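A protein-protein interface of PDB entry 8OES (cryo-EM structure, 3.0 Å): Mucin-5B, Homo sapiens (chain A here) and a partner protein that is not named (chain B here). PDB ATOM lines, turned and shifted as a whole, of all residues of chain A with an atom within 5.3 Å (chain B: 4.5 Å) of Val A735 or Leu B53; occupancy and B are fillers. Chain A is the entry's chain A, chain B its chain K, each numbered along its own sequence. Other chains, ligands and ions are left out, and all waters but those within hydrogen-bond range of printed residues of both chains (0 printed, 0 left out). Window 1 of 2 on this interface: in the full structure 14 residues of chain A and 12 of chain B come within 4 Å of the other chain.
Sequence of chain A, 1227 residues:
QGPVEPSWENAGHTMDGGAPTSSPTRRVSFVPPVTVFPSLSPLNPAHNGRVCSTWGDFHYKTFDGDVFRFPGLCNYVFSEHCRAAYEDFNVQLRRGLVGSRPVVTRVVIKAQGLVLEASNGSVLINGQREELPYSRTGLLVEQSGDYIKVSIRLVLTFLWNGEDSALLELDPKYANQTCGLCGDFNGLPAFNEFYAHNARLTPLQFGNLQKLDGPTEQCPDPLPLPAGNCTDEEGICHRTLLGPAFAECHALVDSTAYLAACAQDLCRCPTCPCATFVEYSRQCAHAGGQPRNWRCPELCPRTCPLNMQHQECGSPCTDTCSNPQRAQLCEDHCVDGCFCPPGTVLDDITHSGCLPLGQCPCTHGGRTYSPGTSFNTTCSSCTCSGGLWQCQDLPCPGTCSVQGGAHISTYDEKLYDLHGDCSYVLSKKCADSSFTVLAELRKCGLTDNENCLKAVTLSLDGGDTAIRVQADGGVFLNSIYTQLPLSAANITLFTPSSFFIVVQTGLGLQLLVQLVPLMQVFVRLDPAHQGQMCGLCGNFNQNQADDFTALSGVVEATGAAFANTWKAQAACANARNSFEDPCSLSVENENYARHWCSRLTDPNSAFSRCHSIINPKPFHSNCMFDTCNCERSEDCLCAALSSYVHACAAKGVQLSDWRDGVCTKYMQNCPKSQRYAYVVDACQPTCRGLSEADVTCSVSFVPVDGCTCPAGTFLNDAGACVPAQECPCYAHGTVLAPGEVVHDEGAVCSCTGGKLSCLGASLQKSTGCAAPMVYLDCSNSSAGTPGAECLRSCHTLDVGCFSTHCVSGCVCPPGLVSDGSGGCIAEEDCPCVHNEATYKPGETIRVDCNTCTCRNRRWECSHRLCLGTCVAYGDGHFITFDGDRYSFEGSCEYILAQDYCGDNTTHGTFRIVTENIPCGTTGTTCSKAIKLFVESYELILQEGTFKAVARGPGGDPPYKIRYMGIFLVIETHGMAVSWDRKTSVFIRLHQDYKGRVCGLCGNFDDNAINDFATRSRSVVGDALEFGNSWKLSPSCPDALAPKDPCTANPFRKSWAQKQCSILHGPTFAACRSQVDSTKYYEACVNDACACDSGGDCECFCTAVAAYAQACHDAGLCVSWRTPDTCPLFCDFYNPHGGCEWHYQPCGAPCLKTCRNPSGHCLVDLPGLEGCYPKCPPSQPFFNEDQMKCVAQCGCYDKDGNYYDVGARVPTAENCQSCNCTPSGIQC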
ATOM      1  N   GLU A 726     -35.109 -13.088 -14.071  1.00  0.00           N
ATOM      2  CA  GLU A 726     -34.434 -14.308 -14.485  1.00  0.00           C
ATOM      3  C   GLU A 726     -33.194 -14.052 -15.330  1.00  0.00           C
ATOM      4  O   GLU A 726     -32.469 -15.005 -15.637  1.00  0.00           O
ATOM      5  CB  GLU A 726     -35.399 -15.202 -15.268  1.00  0.00           C
ATOM      6  CG  GLU A 726     -36.500 -15.823 -14.435  1.00  0.00           C
ATOM      7  CD  GLU A 726     -37.701 -14.913 -14.301  1.00  0.00           C
ATOM      8  OE1 GLU A 726     -37.532 -13.687 -14.440  1.00  0.00           O
ATOM      9  OE2 GLU A 726     -38.815 -15.421 -14.058  1.00  0.00           O
ATOM     10  N   CYS A 727     -32.928 -12.805 -15.710  1.00  0.00           N
ATOM     11  CA  CYS A 727     -31.771 -12.575 -16.553  1.00  0.00           C
ATOM     12  C   CYS A 727     -30.692 -11.827 -15.782  1.00  0.00           C
ATOM     13  O   CYS A 727     -31.006 -10.986 -14.932  1.00  0.00           O
ATOM     14  CB  CYS A 727     -32.151 -11.783 -17.807  1.00  0.00           C
ATOM     15  SG  CYS A 727     -31.803 -10.019 -17.733  1.00  0.00           S
ATOM     16  N   PRO A 728     -29.424 -12.112 -16.049  1.00  0.00           N
ATOM     17  CA  PRO A 728     -28.342 -11.624 -15.193  1.00  0.00           C
ATOM     18  C   PRO A 728     -27.738 -10.305 -15.644  1.00  0.00           C
ATOM     19  O   PRO A 728     -27.717  -9.965 -16.826  1.00  0.00           O
ATOM     20  CB  PRO A 728     -27.302 -12.744 -15.320  1.00  0.00           C
ATOM     21  CG  PRO A 728     -27.467 -13.194 -16.724  1.00  0.00           C
ATOM     22  CD  PRO A 728     -28.940 -13.099 -17.028  1.00  0.00           C
ATOM     23  N   CYS A 729     -27.222  -9.564 -14.669  1.00  0.00           N
ATOM     24  CA  CYS A 729     -26.369  -8.427 -14.980  1.00  0.00           C
ATOM     25  C   CYS A 729     -25.023  -8.915 -15.496  1.00  0.00           C
ATOM     26  O   CYS A 729     -24.545  -9.985 -15.114  1.00  0.00           O
ATOM     27  CB  CYS A 729     -26.176  -7.549 -13.749  1.00  0.00           C
ATOM     28  SG  CYS A 729     -27.617  -7.428 -12.676  1.00  0.00           S
ATOM     29  N   TYR A 730     -24.413  -8.127 -16.380  1.00  0.00           N
ATOM     30  CA  TYR A 730     -23.165  -8.497 -17.040  1.00  0.00           C
ATOM     31  C   TYR A 730     -22.105  -7.443 -16.754  1.00  0.00           C
ATOM     32  O   TYR A 730     -22.234  -6.294 -17.192  1.00  0.00           O
ATOM     33  CB  TYR A 730     -23.374  -8.648 -18.546  1.00  0.00           C
ATOM     34  CG  TYR A 730     -24.278  -9.796 -18.913  1.00  0.00           C
ATOM     35  CD1 TYR A 730     -23.790 -11.090 -18.999  1.00  0.00           C
ATOM     36  CD2 TYR A 730     -25.627  -9.590 -19.146  1.00  0.00           C
ATOM     37  CE1 TYR A 730     -24.617 -12.140 -19.327  1.00  0.00           C
ATOM     38  CE2 TYR A 730     -26.462 -10.636 -19.468  1.00  0.00           C
ATOM     39  CZ  TYR A 730     -25.952 -11.904 -19.560  1.00  0.00           C
ATOM     40  OH  TYR A 730     -26.787 -12.942 -19.886  1.00  0.00           O
ATOM     41  N   GLY A 733     -18.385  -8.417 -19.293  1.00  0.00           N
ATOM     42  CA  GLY A 733     -18.788  -9.579 -20.048  1.00  0.00           C
ATOM     43  C   GLY A 733     -19.009 -10.826 -19.226  1.00  0.00           C
ATOM     44  O   GLY A 733     -19.241 -11.893 -19.805  1.00  0.00           O
ATOM     45  N   THR A 734     -18.948 -10.732 -17.901  1.00  0.00           N
ATOM     46  CA  THR A 734     -19.160 -11.886 -17.038  1.00  0.00           C
ATOM     47  C   THR A 734     -20.631 -12.012 -16.681  1.00  0.00           C
ATOM     48  O   THR A 734     -21.271 -11.041 -16.270  1.00  0.00           O
ATOM     49  CB  THR A 734     -18.333 -11.781 -15.755  1.00  0.00           C
ATOM     50  OG1 THR A 734     -18.652 -10.557 -15.081  1.00  0.00           O
ATOM     51  CG2 THR A 734     -16.849 -11.808 -16.072  1.00  0.00           C
ATOM     52  N   VAL A 735     -21.162 -13.220 -16.844  1.00  0.00           N
ATOM     53  CA  VAL A 735     -22.537 -13.491 -16.454  1.00  0.00           C
ATOM     54  C   VAL A 735     -22.625 -13.436 -14.937  1.00  0.00           C
ATOM     55  O   VAL A 735     -22.114 -14.319 -14.238  1.00  0.00           O
ATOM     56  CB  VAL A 735     -23.000 -14.851 -16.986  1.00  0.00           C
ATOM     57  CG1 VAL A 735     -24.467 -15.066 -16.671  1.00  0.00           C
ATOM     58  CG2 VAL A 735     -22.741 -14.958 -18.478  1.00  0.00           C
ATOM     59  N   LEU A 736     -23.268 -12.397 -14.417  1.00  0.00           N
ATOM     60  CA  LEU A 736     -23.404 -12.214 -12.979  1.00  0.00           C
ATOM     61  C   LEU A 736     -24.878 -12.410 -12.656  1.00  0.00           C
ATOM     62  O   LEU A 736     -25.705 -11.551 -12.978  1.00  0.00           O
ATOM     63  CB  LEU A 736     -22.906 -10.836 -12.549  1.00  0.00           C
ATOM     64  CG  LEU A 736     -22.712 -10.595 -11.054  1.00  0.00           C
ATOM     65  CD1 LEU A 736     -23.997 -10.229 -10.333  1.00  0.00           C
ATOM     66  CD2 LEU A 736     -22.064 -11.817 -10.446  1.00  0.00           C
ATOM     67  N   ALA A 737     -25.193 -13.521 -12.000  1.00  0.00           N
ATOM     68  CA  ALA A 737     -26.563 -14.005 -11.931  1.00  0.00           C
ATOM     69  C   ALA A 737     -27.460 -13.038 -11.155  1.00  0.00           C
ATOM     70  O   ALA A 737     -26.981 -12.247 -10.338  1.00  0.00           O
ATOM     71  CB  ALA A 737     -26.591 -15.384 -11.282  1.00  0.00           C
ATOM     72  N   PRO A 738     -28.768 -13.071 -11.408  1.00  0.00           N
ATOM     73  CA  PRO A 738     -29.674 -12.132 -10.739  1.00  0.00           C
ATOM     74  C   PRO A 738     -29.741 -12.373  -9.240  1.00  0.00           C
ATOM     75  O   PRO A 738     -29.599 -13.500  -8.761  1.00  0.00           O
ATOM     76  CB  PRO A 738     -31.028 -12.413 -11.398  1.00  0.00           C
ATOM     77  CG  PRO A 738     -30.719 -13.132 -12.650  1.00  0.00           C
ATOM     78  CD  PRO A 738     -29.473 -13.903 -12.396  1.00  0.00           C
ATOM     79  N   GLU A 740     -27.732 -11.618  -6.861  1.00  0.00           N
ATOM     80  CA  GLU A 740     -26.492 -12.192  -6.362  1.00  0.00           C
ATOM     81  C   GLU A 740     -25.555 -11.076  -5.935  1.00  0.00           C
ATOM     82  O   GLU A 740     -25.213 -10.202  -6.739  1.00  0.00           O
ATOM     83  CB  GLU A 740     -25.837 -13.074  -7.427  1.00  0.00           C
ATOM     84  CG  GLU A 740     -24.339 -13.222  -7.292  1.00  0.00           C
ATOM     85  CD  GLU A 740     -23.727 -13.931  -8.481  1.00  0.00           C
ATOM     86  OE1 GLU A 740     -24.344 -13.910  -9.565  1.00  0.00           O
ATOM     87  OE2 GLU A 740     -22.628 -14.504  -8.340  1.00  0.00           O
ATOM     88  N   ALA B  50     -27.297 -23.926 -14.536  1.00  0.00           N
ATOM     89  CA  ALA B  50     -27.542 -22.961 -13.477  1.00  0.00           C
ATOM     90  C   ALA B  50     -29.034 -22.905 -13.176  1.00  0.00           C
ATOM     91  O   ALA B  50     -29.854 -22.763 -14.086  1.00  0.00           O
ATOM     92  CB  ALA B  50     -27.026 -21.579 -13.876  1.00  0.00           C
ATOM     93  N   ALA B  51     -29.385 -23.022 -11.893  1.00  0.00           N
ATOM     94  CA  ALA B  51     -30.793 -23.086 -11.513  1.00  0.00           C
ATOM     95  C   ALA B  51     -31.502 -21.755 -11.740  1.00  0.00           C
ATOM     96  O   ALA B  51     -32.661 -21.731 -12.170  1.00  0.00           O
ATOM     97  CB  ALA B  51     -30.922 -23.520 -10.056  1.00  0.00           C
ATOM     98  N   GLN B  52     -30.832 -20.637 -11.453  1.00  0.00           N
ATOM     99  CA  GLN B  52     -31.447 -19.321 -11.596  1.00  0.00           C
ATOM    100  C   GLN B  52     -31.410 -18.790 -13.026  1.00  0.00           C
ATOM    101  O   GLN B  52     -32.119 -17.826 -13.330  1.00  0.00           O
ATOM    102  CB  GLN B  52     -30.767 -18.321 -10.659  1.00  0.00           C
ATOM    103  CG  GLN B  52     -31.580 -17.072 -10.392  1.00  0.00           C
ATOM    104  CD  GLN B  52     -30.768 -15.983  -9.730  1.00  0.00           C
ATOM    105  OE1 GLN B  52     -29.546 -15.957  -9.832  1.00  0.00           O
ATOM    106  NE2 GLN B  52     -31.447 -15.069  -9.046  1.00  0.00           N
ATOM    107  N   LEU B  53     -30.610 -19.389 -13.908  1.00  0.00           N
ATOM    108  CA  LEU B  53     -30.537 -18.994 -15.314  1.00  0.00           C
ATOM    109  C   LEU B  53     -30.765 -20.239 -16.155  1.00  0.00           C
ATOM    110  O   LEU B  53     -29.808 -20.881 -16.610  1.00  0.00           O
ATOM    111  CB  LEU B  53     -29.199 -18.338 -15.642  1.00  0.00           C
ATOM    112  CG  LEU B  53     -28.817 -17.149 -14.764  1.00  0.00           C
ATOM    113  CD1 LEU B  53     -27.437 -16.635 -15.130  1.00  0.00           C
ATOM    114  CD2 LEU B  53     -29.852 -16.049 -14.886  1.00  0.00           C
ATOM    115  N   PRO B  54     -32.023 -20.612 -16.388  1.00  0.00           N
ATOM    116  CA  PRO B  54     -32.325 -21.889 -17.042  1.00  0.00           C
ATOM    117  C   PRO B  54     -32.235 -21.869 -18.560  1.00  0.00           C
ATOM    118  O   PRO B  54     -32.702 -22.818 -19.194  1.00  0.00           O
ATOM    119  CB  PRO B  54     -33.766 -22.159 -16.589  1.00  0.00           C
ATOM    120  CG  PRO B  54     -34.356 -20.802 -16.399  1.00  0.00           C
ATOM    121  CD  PRO B  54     -33.239 -19.849 -16.062  1.00  0.00           C
ATOM    122  N   ASP B  55     -31.659 -20.831 -19.161  1.00  0.00           N
ATOM    123  CA  ASP B  55     -31.540 -20.741 -20.611  1.00  0.00           C
ATOM    124  C   ASP B  55     -30.100 -20.791 -21.094  1.00  0.00           C
ATOM    125  O   ASP B  55     -29.754 -21.645 -21.916  1.00  0.00           O
ATOM    126  CB  ASP B  55     -32.193 -19.449 -21.114  1.00  0.00           C
ATOM    127  CG  ASP B  55     -33.674 -19.394 -20.830  1.00  0.00           C
ATOM    128  OD1 ASP B  55     -34.221 -20.388 -20.305  1.00  0.00           O
ATOM    129  OD2 ASP B  55     -34.292 -18.353 -21.137  1.00  0.00           O
ATOM    130  N   MET B  56     -29.254 -19.891 -20.610  1.00  0.00           N
ATOM    131  CA  MET B  56     -27.901 -19.795 -21.132  1.00  0.00           C
ATOM    132  C   MET B  56     -27.050 -20.962 -20.635  1.00  0.00           C
ATOM    133  O   MET B  56     -26.976 -21.212 -19.428  1.00  0.00           O
ATOM    134  CB  MET B  56     -27.276 -18.461 -20.736  1.00  0.00           C
ATOM    135  CG  MET B  56     -27.573 -18.030 -19.316  1.00  0.00           C
ATOM    136  SD  MET B  56     -26.243 -17.027 -18.645  1.00  0.00           S
ATOM    137  CE  MET B  56     -25.998 -15.879 -19.996  1.00  0.00           C
ATOM    138  N   GLU B  60     -21.551 -20.705 -21.953  1.00  0.00           N
ATOM    139  CA  GLU B  60     -21.858 -19.286 -22.088  1.00  0.00           C
ATOM    140  C   GLU B  60     -21.623 -18.541 -20.782  1.00  0.00           C
ATOM    141  O   GLU B  60     -21.350 -17.336 -20.798  1.00  0.00           O
ATOM    142  CB  GLU B  60     -23.301 -19.103 -22.557  1.00  0.00           C
ATOM    143  CG  GLU B  60     -23.524 -19.434 -24.027  1.00  0.00           C
ATOM    144  CD  GLU B  60     -23.410 -18.223 -24.932  1.00  0.00           C
ATOM    145  OE1 GLU B  60     -22.746 -17.242 -24.539  1.00  0.00           O
ATOM    146  OE2 GLU B  60     -23.993 -18.254 -26.036  1.00  0.00           O
ATOM    147  N   LEU B  61     -21.741 -19.231 -19.644  1.00  0.00           N
ATOM    148  CA  LEU B  61     -21.415 -18.612 -18.365  1.00  0.00           C
ATOM    149  C   LEU B  61     -19.940 -18.243 -18.301  1.00  0.00           C
ATOM    150  O   LEU B  61     -19.578 -17.139 -17.884  1.00  0.00           O
ATOM    151  CB  LEU B  61     -21.773 -19.552 -17.212  1.00  0.00           C
ATOM    152  CG  LEU B  61     -23.233 -19.874 -16.897  1.00  0.00           C
ATOM    153  CD1 LEU B  61     -23.300 -20.878 -15.761  1.00  0.00           C
ATOM    154  CD2 LEU B  61     -23.997 -18.619 -16.534  1.00  0.00           C
ATOM    155  N   GLN B  63     -17.806 -19.594 -16.291  1.00  0.00           N
ATOM    156  CA  GLN B  63     -17.273 -19.854 -14.963  1.00  0.00           C
ATOM    157  C   GLN B  63     -16.649 -21.243 -14.905  1.00  0.00           C
ATOM    158  O   GLN B  63     -16.937 -22.118 -15.723  1.00  0.00           O
ATOM    159  CB  GLN B  63     -18.361 -19.729 -13.891  1.00  0.00           C
ATOM    160  CG  GLN B  63     -19.588 -18.853 -14.203  1.00  0.00           C
ATOM    161  CD  GLN B  63     -19.299 -17.517 -14.889  1.00  0.00           C
ATOM    162  OE1 GLN B  63     -18.159 -17.060 -14.976  1.00  0.00           O
ATOM    163  NE2 GLN B  63     -20.355 -16.885 -15.382  1.00  0.00           N
ATOM    164  N   HIS B  86     -22.574 -19.292  -9.078  1.00  0.00           N
ATOM    165  CA  HIS B  86     -24.017 -19.239  -9.229  1.00  0.00           C
ATOM    166  C   HIS B  86     -24.629 -20.451  -8.534  1.00  0.00           C
ATOM    167  O   HIS B  86     -23.925 -21.335  -8.046  1.00  0.00           O
ATOM    168  CB  HIS B  86     -24.389 -19.180 -10.707  1.00  0.00           C
ATOM    169  CG  HIS B  86     -23.748 -18.047 -11.445  1.00  0.00           C
ATOM    170  ND1 HIS B  86     -23.073 -18.219 -12.635  1.00  0.00           N
ATOM    171  CD2 HIS B  86     -23.669 -16.726 -11.156  1.00  0.00           C
ATOM    172  CE1 HIS B  86     -22.616 -17.051 -13.051  1.00  0.00           C
ATOM    173  NE2 HIS B  86     -22.964 -16.129 -12.173  1.00  0.00           N
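O of Val A735 sits at hydrogen-bond distance from NE2 of His B86 (2.9 Å). A ring nitrogen (NE2) of His B86 lies within hydrogen-bond range of the backbone NH (N) of Ala A737, 3.4 Å away. NE2 of Gln B63 lies within hydrogen-bond range of O of Val A735 (3.3 Å). O of Pro A738 is in hydrogen-bond range of NE2 of Gln B52.
OE1 of Glu A740 is in hydrogen-bond range of N of Ala A737, 2.6 Å away. The backbone carbonyl oxygen of Leu B61 lies within hydrogen-bond range of the side-chain amide nitrogen of Gln B63, at 2.6 Å.
Among the printed residues, pairs that only touch across the chains: Glu A726 with Gln B52 (3.7 Å), Glu A726 with Leu B53 (2.9 Å), Pro A728 with Leu B53 (3.8 Å), Tyr A730 with Met B56 (3.0 Å), Val A735 with Leu B53 (3.7 Å), Val A735 with Met B56 (3.3 Å), Val A735 with Glu B60 (3.6 Å), Val A735 with Leu B61 (3.6 Å), Ala A737 with Gln B52 (3.3 Å), Pro A738 with Leu B53 (3.3 Å) and Glu A740 with His B86 (3.3 Å).
Cys A727 touches none of the printed residues of chain B. Printed residues of chain B within 4 Å of Tyr A730: Met B56. Thr A734 touches none of the printed residues of chain B. Val A735 touches six residues of chain B. Leu B53 touches four residues of chain A. Printed residues of chain A within 4 Å of Gln B63: Val A735 (3.3 Å). The nearest printed residue of chain B that does not touch Val A735 is Ala B50 (7.5 Å). The nearest printed residue of chain A that does not touch Leu B61 is Thr A734 (5.3 Å).
Hydrophobic or aromatic side chains of chain A that line the printed part of chain B: Pro A728, Tyr A730, Val A735, Ala A737 and Pro A738. Hydrophobic or aromatic side chains of chain B within 4 Å of the printed part of chain A: Leu B53, Met B56, Leu B61 and His B86.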
